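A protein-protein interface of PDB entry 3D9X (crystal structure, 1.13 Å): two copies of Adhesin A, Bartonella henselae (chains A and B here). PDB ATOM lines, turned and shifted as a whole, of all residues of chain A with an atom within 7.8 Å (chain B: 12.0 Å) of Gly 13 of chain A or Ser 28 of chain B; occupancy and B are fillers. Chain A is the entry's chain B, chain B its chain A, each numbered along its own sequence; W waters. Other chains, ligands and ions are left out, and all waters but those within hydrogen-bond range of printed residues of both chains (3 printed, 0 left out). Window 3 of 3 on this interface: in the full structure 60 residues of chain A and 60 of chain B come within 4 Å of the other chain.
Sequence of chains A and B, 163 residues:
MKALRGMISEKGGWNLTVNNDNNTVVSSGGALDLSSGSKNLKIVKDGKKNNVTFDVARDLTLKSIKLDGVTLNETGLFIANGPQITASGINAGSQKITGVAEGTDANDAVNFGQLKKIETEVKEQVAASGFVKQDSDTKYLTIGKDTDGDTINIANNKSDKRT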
ATOM      1  N   GLY A  12     -12.632  21.464 -18.242  1.00  0.00           N
ATOM      2  CA  GLY A  12     -11.261  21.902 -18.021  1.00  0.00           C
ATOM      3  C   GLY A  12     -10.253  20.773 -18.100  1.00  0.00           C
ATOM      4  O   GLY A  12      -9.623  20.581 -19.145  1.00  0.00           O
ATOM      5  N   GLY A  13     -10.090  20.001 -17.023  1.00  0.00           N
ATOM      6  CA  GLY A  13     -10.860  20.123 -15.774  1.00  0.00           C
ATOM      7  C   GLY A  13     -11.128  18.749 -15.201  1.00  0.00           C
ATOM      8  O   GLY A  13     -11.003  17.746 -15.903  1.00  0.00           O
ATOM      9  N   TRP A  14     -11.526  18.703 -13.934  1.00  0.00           N
ATOM     10  CA  TRP A  14     -11.824  17.444 -13.260  1.00  0.00           C
ATOM     11  C   TRP A  14     -13.266  17.475 -12.761  1.00  0.00           C
ATOM     12  O   TRP A  14     -13.856  18.527 -12.551  1.00  0.00           O
ATOM     13  CB  TRP A  14     -10.823  17.170 -12.123  1.00  0.00           C
ATOM     14  CG  TRP A  14     -10.738  18.235 -11.092  1.00  0.00           C
ATOM     15  CD1 TRP A  14     -10.025  19.405 -11.151  1.00  0.00           C
ATOM     16  CD2 TRP A  14     -11.396  18.235  -9.819  1.00  0.00           C
ATOM     17  NE1 TRP A  14     -10.203  20.123  -9.999  1.00  0.00           N
ATOM     18  CE2 TRP A  14     -11.032  19.428  -9.161  1.00  0.00           C
ATOM     19  CE3 TRP A  14     -12.245  17.339  -9.161  1.00  0.00           C
ATOM     20  CZ2 TRP A  14     -11.495  19.743  -7.887  1.00  0.00           C
ATOM     21  CZ3 TRP A  14     -12.701  17.654  -7.895  1.00  0.00           C
ATOM     22  CH2 TRP A  14     -12.324  18.852  -7.270  1.00  0.00           C
ATOM     23  N   ASN A  15     -13.828  16.295 -12.592  1.00  0.00           N
ATOM     24  CA  ASN A  15     -15.246  16.131 -12.280  1.00  0.00           C
ATOM     25  C   ASN A  15     -15.418  15.902 -10.796  1.00  0.00           C
ATOM     26  O   ASN A  15     -14.686  15.111 -10.217  1.00  0.00           O
ATOM     27  CB  ASN A  15     -15.795  14.947 -13.054  1.00  0.00           C
ATOM     28  CG  ASN A  15     -15.834  15.206 -14.547  1.00  0.00           C
ATOM     29  OD1 ASN A  15     -16.763  15.831 -15.038  1.00  0.00           O
ATOM     30  ND2 ASN A  15     -14.831  14.726 -15.269  1.00  0.00           N
ATOM     31  N   LEU A  16     -16.368  16.605 -10.196  1.00  0.00           N
ATOM     32  CA  LEU A  16     -16.659  16.495  -8.774  1.00  0.00           C
ATOM     33  C   LEU A  16     -18.109  16.076  -8.582  1.00  0.00           C
ATOM     34  O   LEU A  16     -19.006  16.735  -9.096  1.00  0.00           O
ATOM     35  CB  LEU A  16     -16.444  17.844  -8.100  1.00  0.00           C
ATOM     36  CG  LEU A  16     -16.806  17.911  -6.610  1.00  0.00           C
ATOM     37  CD1 LEU A  16     -15.972  16.973  -5.770  1.00  0.00           C
ATOM     38  CD2 LEU A  16     -16.647  19.345  -6.139  1.00  0.00           C
ATOM     39  N   THR A  24     -20.223  18.258 -11.441  1.00  0.00           N
ATOM     40  CA  THR A  24     -19.829  19.427 -12.213  1.00  0.00           C
ATOM     41  C   THR A  24     -18.348  19.326 -12.505  1.00  0.00           C
ATOM     42  O   THR A  24     -17.607  18.583 -11.870  1.00  0.00           O
ATOM     43  CB  THR A  24     -20.104  20.758 -11.495  1.00  0.00           C
ATOM     44  OG1 THR A  24     -19.485  20.732 -10.210  1.00  0.00           O
ATOM     45  CG2 THR A  24     -21.599  21.052 -11.340  1.00  0.00           C
ATOM     46  N   VAL A  25     -17.941  20.076 -13.511  1.00  0.00           N
ATOM     47  CA  VAL A  25     -16.535  20.172 -13.878  1.00  0.00           C
ATOM     48  C   VAL A  25     -15.909  21.371 -13.188  1.00  0.00           C
ATOM     49  O   VAL A  25     -16.385  22.505 -13.298  1.00  0.00           O
ATOM     50  CB  VAL A  25     -16.371  20.311 -15.400  1.00  0.00           C
ATOM     51  CG1 VAL A  25     -14.885  20.438 -15.778  1.00  0.00           C
ATOM     52  CG2 VAL A  25     -17.006  19.147 -16.110  1.00  0.00           C
ATOM     53  N   VAL A  26     -14.817  21.102 -12.484  1.00  0.00           N
ATOM     54  CA  VAL A  26     -13.966  22.141 -11.940  1.00  0.00           C
ATOM     55  C   VAL A  26     -12.937  22.377 -13.054  1.00  0.00           C
ATOM     56  O   VAL A  26     -12.030  21.572 -13.257  1.00  0.00           O
ATOM     57  CB  VAL A  26     -13.334  21.705 -10.611  1.00  0.00           C
ATOM     58  CG1 VAL A  26     -12.472  22.818 -10.034  1.00  0.00           C
ATOM     59  CG2 VAL A  26     -14.428  21.327  -9.626  1.00  0.00           C
ATOM     60  N   SER A  27     -13.149  23.449 -13.823  1.00  0.00           N
ATOM     61  CA  SER A  27     -12.349  23.741 -15.009  1.00  0.00           C
ATOM     62  C   SER A  27     -11.013  24.320 -14.621  1.00  0.00           C
ATOM     63  O   SER A  27     -10.827  24.817 -13.500  1.00  0.00           O
ATOM     64  CB  SER A  27     -13.079  24.729 -15.919  1.00  0.00           C
ATOM     65  OG  SER A  27     -13.317  25.941 -15.248  1.00  0.00           O
ATOM     66  N   SER A  28     -10.097  24.292 -15.586  1.00  0.00           N
ATOM     67  CA  SER A  28      -8.838  24.991 -15.475  1.00  0.00           C
ATOM     68  C   SER A  28      -9.132  26.466 -15.245  1.00  0.00           C
ATOM     69  O   SER A  28      -9.881  27.083 -16.006  1.00  0.00           O
ATOM     70  CB  SER A  28      -8.032  24.822 -16.759  1.00  0.00           C
ATOM     71  OG  SER A  28      -6.737  25.355 -16.601  1.00  0.00           O
ATOM     72  N   GLY A  29      -8.577  27.026 -14.178  1.00  0.00           N
ATOM     73  CA  GLY A  29      -8.883  28.386 -13.773  1.00  0.00           C
ATOM     74  C   GLY A  29     -10.225  28.564 -13.079  1.00  0.00           C
ATOM     75  O   GLY A  29     -10.627  29.684 -12.792  1.00  0.00           O
ATOM     76  N   GLY B  12      -2.110  17.111 -15.485  1.00  0.00           N
ATOM     77  CA  GLY B  12      -2.673  18.129 -14.548  1.00  0.00           C
ATOM     78  C   GLY B  12      -4.140  17.904 -14.220  1.00  0.00           C
ATOM     79  O   GLY B  12      -5.008  18.511 -14.852  1.00  0.00           O
ATOM     80  N   GLY B  13      -4.451  17.033 -13.254  1.00  0.00           N
ATOM     81  CA  GLY B  13      -3.470  16.275 -12.522  1.00  0.00           C
ATOM     82  C   GLY B  13      -3.066  17.073 -11.307  1.00  0.00           C
ATOM     83  O   GLY B  13      -2.155  17.911 -11.377  1.00  0.00           O
ATOM     84  N   TRP B  14      -3.793  16.847 -10.209  1.00  0.00           N
ATOM     85  CA  TRP B  14      -3.384  17.303  -8.887  1.00  0.00           C
ATOM     86  C   TRP B  14      -3.469  16.112  -7.935  1.00  0.00           C
ATOM     87  O   TRP B  14      -4.140  15.119  -8.213  1.00  0.00           O
ATOM     88  CB  TRP B  14      -4.225  18.502  -8.421  1.00  0.00           C
ATOM     89  CG  TRP B  14      -5.697  18.257  -8.392  1.00  0.00           C
ATOM     90  CD1 TRP B  14      -6.555  18.295  -9.453  1.00  0.00           C
ATOM     91  CD2 TRP B  14      -6.482  17.917  -7.251  1.00  0.00           C
ATOM     92  NE1 TRP B  14      -7.837  18.007  -9.034  1.00  0.00           N
ATOM     93  CE2 TRP B  14      -7.819  17.789  -7.682  1.00  0.00           C
ATOM     94  CE3 TRP B  14      -6.191  17.734  -5.899  1.00  0.00           C
ATOM     95  CZ2 TRP B  14      -8.859  17.490  -6.803  1.00  0.00           C
ATOM     96  CZ3 TRP B  14      -7.214  17.422  -5.033  1.00  0.00           C
ATOM     97  CH2 TRP B  14      -8.539  17.299  -5.490  1.00  0.00           C
ATOM     98  N   ASN B  15      -2.754  16.219  -6.836  1.00  0.00           N
ATOM     99  CA  ASN B  15      -2.677  15.152  -5.832  1.00  0.00           C
ATOM    100  C   ASN B  15      -3.588  15.428  -4.653  1.00  0.00           C
ATOM    101  O   ASN B  15      -3.586  16.516  -4.110  1.00  0.00           O
ATOM    102  CB  ASN B  15      -1.257  15.028  -5.314  1.00  0.00           C
ATOM    103  CG  ASN B  15      -0.283  14.658  -6.404  1.00  0.00           C
ATOM    104  OD1 ASN B  15      -0.288  13.535  -6.883  1.00  0.00           O
ATOM    105  ND2 ASN B  15       0.527  15.622  -6.842  1.00  0.00           N
ATOM    106  N   LEU B  16      -4.354  14.424  -4.260  1.00  0.00           N
ATOM    107  CA  LEU B  16      -5.189  14.476  -3.087  1.00  0.00           C
ATOM    108  C   LEU B  16      -4.643  13.542  -2.012  1.00  0.00           C
ATOM    109  O   LEU B  16      -4.393  12.377  -2.302  1.00  0.00           O
ATOM    110  CB  LEU B  16      -6.610  14.050  -3.446  1.00  0.00           C
ATOM    111  CG  LEU B  16      -7.607  13.980  -2.287  1.00  0.00           C
ATOM    112  CD1 LEU B  16      -7.837  15.324  -1.652  1.00  0.00           C
ATOM    113  CD2 LEU B  16      -8.897  13.392  -2.811  1.00  0.00           C
ATOM    114  N   THR B  24      -3.386  10.382  -4.136  1.00  0.00           N
ATOM    115  CA  THR B  24      -4.275   9.857  -5.154  1.00  0.00           C
ATOM    116  C   THR B  24      -4.375  10.940  -6.218  1.00  0.00           C
ATOM    117  O   THR B  24      -4.727  12.081  -5.903  1.00  0.00           O
ATOM    118  CB  THR B  24      -5.669   9.550  -4.587  1.00  0.00           C
ATOM    119  OG1 THR B  24      -5.554   8.511  -3.619  1.00  0.00           O
ATOM    120  CG2 THR B  24      -6.650   9.141  -5.673  1.00  0.00           C
ATOM    121  N   VAL B  25      -4.074  10.619  -7.475  1.00  0.00           N
ATOM    122  CA  VAL B  25      -4.106  11.620  -8.521  1.00  0.00           C
ATOM    123  C   VAL B  25      -5.516  11.813  -9.013  1.00  0.00           C
ATOM    124  O   VAL B  25      -6.255  10.855  -9.244  1.00  0.00           O
ATOM    125  CB  VAL B  25      -3.247  11.257  -9.730  1.00  0.00           C
ATOM    126  CG1 VAL B  25      -3.186  12.438 -10.678  1.00  0.00           C
ATOM    127  CG2 VAL B  25      -1.879  10.887  -9.311  1.00  0.00           C
ATOM    128  N   VAL B  26      -5.891  13.075  -9.135  1.00  0.00           N
ATOM    129  CA  VAL B  26      -7.117  13.458  -9.801  1.00  0.00           C
ATOM    130  C   VAL B  26      -6.634  14.058 -11.108  1.00  0.00           C
ATOM    131  O   VAL B  26      -6.129  15.172 -11.154  1.00  0.00           O
ATOM    132  CB  VAL B  26      -7.936  14.441  -8.959  1.00  0.00           C
ATOM    133  CG1 VAL B  26      -9.203  14.844  -9.707  1.00  0.00           C
ATOM    134  CG2 VAL B  26      -8.267  13.813  -7.615  1.00  0.00           C
ATOM    135  N   SER B  27      -6.748  13.261 -12.168  1.00  0.00           N
ATOM    136  CA  SER B  27      -6.179  13.582 -13.465  1.00  0.00           C
ATOM    137  C   SER B  27      -7.025  14.597 -14.199  1.00  0.00           C
ATOM    138  O   SER B  27      -8.196  14.801 -13.884  1.00  0.00           O
ATOM    139  CB  SER B  27      -6.096  12.309 -14.323  1.00  0.00           C
ATOM    140  OG  SER B  27      -7.387  11.789 -14.616  1.00  0.00           O
ATOM    141  N   SER B  28      -6.425  15.212 -15.215  1.00  0.00           N
ATOM    142  CA  SER B  28      -7.160  15.996 -16.184  1.00  0.00           C
ATOM    143  C   SER B  28      -8.276  15.129 -16.786  1.00  0.00           C
ATOM    144  O   SER B  28      -8.027  14.046 -17.316  1.00  0.00           O
ATOM    145  CB  SER B  28      -6.203  16.460 -17.282  1.00  0.00           C
ATOM    146  OG  SER B  28      -6.795  17.411 -18.132  1.00  0.00           O
ATOM    147  N   GLY B  29      -9.514  15.577 -16.670  1.00  0.00           N
ATOM    148  CA  GLY B  29     -10.656  14.798 -17.125  1.00  0.00           C
ATOM    149  C   GLY B  29     -11.076  13.680 -16.178  1.00  0.00           C
ATOM    150  O   GLY B  29     -12.017  12.936 -16.471  1.00  0.00           O
ATOM    151  N   GLY B  30     -10.381  13.555 -15.049  1.00  0.00           N
ATOM    152  CA  GLY B  30     -10.690  12.557 -14.033  1.00  0.00           C
ATOM    153  C   GLY B  30     -11.807  12.998 -13.113  1.00  0.00           C
ATOM    154  O   GLY B  30     -12.535  13.941 -13.417  1.00  0.00           O
ATOM    155  N   ALA B  31     -11.927  12.316 -11.987  1.00  0.00           N
ATOM    156  CA  ALA B  31     -13.074  12.490 -11.118  1.00  0.00           C
ATOM    157  C   ALA B  31     -12.709  12.296  -9.658  1.00  0.00           C
ATOM    158  O   ALA B  31     -11.769  11.565  -9.317  1.00  0.00           O
ATOM    159  CB  ALA B  31     -14.192  11.505 -11.524  1.00  0.00           C
ATOM    160  N   LEU B  32     -13.495  12.941  -8.815  1.00  0.00           N
ATOM    161  CA  LEU B  32     -13.426  12.770  -7.382  1.00  0.00           C
ATOM    162  C   LEU B  32     -14.851  12.782  -6.848  1.00  0.00           C
ATOM    163  O   LEU B  32     -15.637  13.672  -7.211  1.00  0.00           O
ATOM    164  CB  LEU B  32     -12.633  13.921  -6.767  1.00  0.00           C
ATOM    165  CG  LEU B  32     -12.557  13.962  -5.240  1.00  0.00           C
ATOM    166  CD1 LEU B  32     -11.898  12.722  -4.682  1.00  0.00           C
ATOM    167  CD2 LEU B  32     -11.831  15.197  -4.779  1.00  0.00           C
ATOM    168  N   ASN B  50     -19.864  24.495  -8.410  1.00  0.00           N
ATOM    169  CA  ASN B  50     -18.947  23.536  -7.781  1.00  0.00           C
ATOM    170  C   ASN B  50     -19.111  23.376  -6.257  1.00  0.00           C
ATOM    171  O   ASN B  50     -18.720  22.342  -5.714  1.00  0.00           O
ATOM    172  CB  ASN B  50     -17.513  23.860  -8.207  1.00  0.00           C
ATOM    173  CG  ASN B  50     -17.305  23.707  -9.705  1.00  0.00           C
ATOM    174  OD1 ASN B  50     -17.866  22.818 -10.333  1.00  0.00           O
ATOM    175  ND2 ASN B  50     -16.467  24.563 -10.270  1.00  0.00           N
HETATM  176  O   HOH W   1     -18.699  24.107 -12.808  1.00  0.00           O
HETATM  177  O   HOH W   2     -14.007  11.382 -15.312  1.00  0.00           O
HETATM  178  O   HOH W   3     -15.429  25.178 -12.961  1.00  0.00           O
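Hydrophobic or aromatic side chains of chain B within 4 Å of the printed part of chain A: Trp 14, Val 26, Ala 31 and Leu 32.
Along chain B the printed residues that touch a printed residue of chain A span positions 14 to 50.
Of the 11 printed residues of chain A, 7 touch a printed residue of chain B.
Printed residues of chain A that touch a printed residue of chain B: Gly 13, Trp 14, Asn 15, Leu 16, Thr 24, Val 25 and Val 26.
Hydrophobic or aromatic side chains of chain A within 4 Å of the printed part of chain B: Trp 14, Leu 16 and Val 26.
Among the printed residues, no Asp or Glu carboxylate lies within 4 Å of a Lys or Arg side-chain nitrogen of the other chain.
The backbone carbonyl oxygen of Gly 13 of chain A sits at hydrogen-bond distance from the backbone NH of Gly 29 of chain B (2.7 Å).
The backbone carbonyl oxygen of Gly 30 of chain B lies within hydrogen-bond range of the backbone NH of Asn 15 of chain A, at 2.8 Å.
N of Leu 32 of chain B lies within hydrogen-bond range of O of Asn 15 of chain A.
The side-chain amide oxygen (OD1) of Asn 50 of chain B lies within hydrogen-bond range of the side-chain hydroxyl (OG1) of Thr 24 of chain A, at 2.6 Å.
O of Val 25 of chain A lies close to OD1 of Asn 50 of chain B (3.3 Å).
The indole nitrogen (NE1) of Trp 14 of chain B lies close to the indole nitrogen (NE1) of Trp 14 of chain A.
Gly 13 of chain A touches Gly 29 of chain B, but with the chains exchanged Gly 29 of chain A does not touch Gly 13 of chain B (10.9 Å).
Trp 14 of chain A touches its own counterpart, Trp 14 of chain B.
Trp 14 of chain A touches Ser 27 of chain B, but with the chains exchanged Ser 27 of chain A does not touch Trp 14 of chain B (8.7 Å).
Asn 15 of chain A touches Gly 29 of chain B, but with the chains exchanged Gly 29 of chain A does not touch Asn 15 of chain B (14.3 Å).
Of the 16 pairs that touch across the chains among the printed residues, 1 has its exchanged pair printed and touching as well.
No residue of chain B comes within 4 Å of Gly 12 of chain A.
Of chain B, only Ser 28 (3.9 Å) and Gly 29 (2.7 Å) come within 4 Å of Gly 13 of chain A.
Of chain B, only Gly 29 (3.5 Å), Gly 30 (2.8 Å), Ala 31 (3.2 Å) and Leu 32 (2.8 Å) come within 4 Å of Asn 15 of chain A.
Of the printed residues of chain B, Thr 24 of chain A touches Asn 50 (2.6 Å).
Val 26 of chain A touches just one residue of chain B: Asn 50 (3.7 Å).
No residue of chain B comes within 4 Å of Ser 27 of chain A.
Ser 28 of chain A touches none of the printed residues of chain B.
Leu 16 of chain B touches none of the printed residues of chain A.
Printed residues of chain A within 4 Å of Val 26 of chain B: Trp 14.
Of the printed residues of chain A, Ser 28 of chain B touches Gly 13.
The nearest residue of chain B that does not touch Gly 13 of chain A is Gly 30 of chain B (4.3 Å).
The nearest printed residue of chain A that does not touch Ala 31 of chain B is Trp 14 of chain A (5.0 Å).
The backbone NH of Gly 13 of chain B sits close to the backbone carbonyl oxygen of Val 26 of chain B (3.3 Å).
The backbone NH (N) of Val 26 of chain B sits at hydrogen-bond distance from the backbone carbonyl oxygen (O) of Trp 14 of chain B.
The backbone NH of Val 26 of chain A lies within hydrogen-bond range of the backbone carbonyl oxygen of Trp 14 of chain A, 2.7 Å away.
N of Leu 16 of chain A lies within hydrogen-bond range of O of Thr 24 of chain A (2.9 Å).
Water W2 lies within hydrogen-bond range of the backbone carbonyl oxygen (O) of Gly 29 of chain B (2.8 Å) and the side-chain amide nitrogen (ND2) of Asn 15 of chain A (3.4 Å).
Water W1 lies within hydrogen-bond range of O of Val 25 of chain A (2.9 Å) and OD1 of Asn 50 of chain B (2.9 Å).
Water W3 lies within hydrogen-bond range of O of Val 25 of chain A (2.9 Å), ND2 of Asn 50 of chain B (2.9 Å) and N of Ser 27 of chain A (3.0 Å).
Among the printed residues, merely in contact across the chains: Asn 15 of chain A with Ala 31 of chain B (3.2 Å), Leu 16 of chain A with Leu 32 of chain B (3.4 Å), Asn 15 of chain A with Gly 29 of chain B (3.5 Å), Trp 14 of chain A with Gly 30 of chain B (3.6 Å), Leu 16 of chain A with Asn 50 of chain B (3.7 Å), Trp 14 of chain A with Val 26 of chain B (3.7 Å), Val 26 of chain A with Asn 50 of chain B (3.7 Å), Gly 13 of chain A with Ser 28 of chain B (3.9 Å), Trp 14 of chain A with Leu 32 of chain B (3.9 Å) and Trp 14 of chain A with Ser 27 of chain B (3.95 Å).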
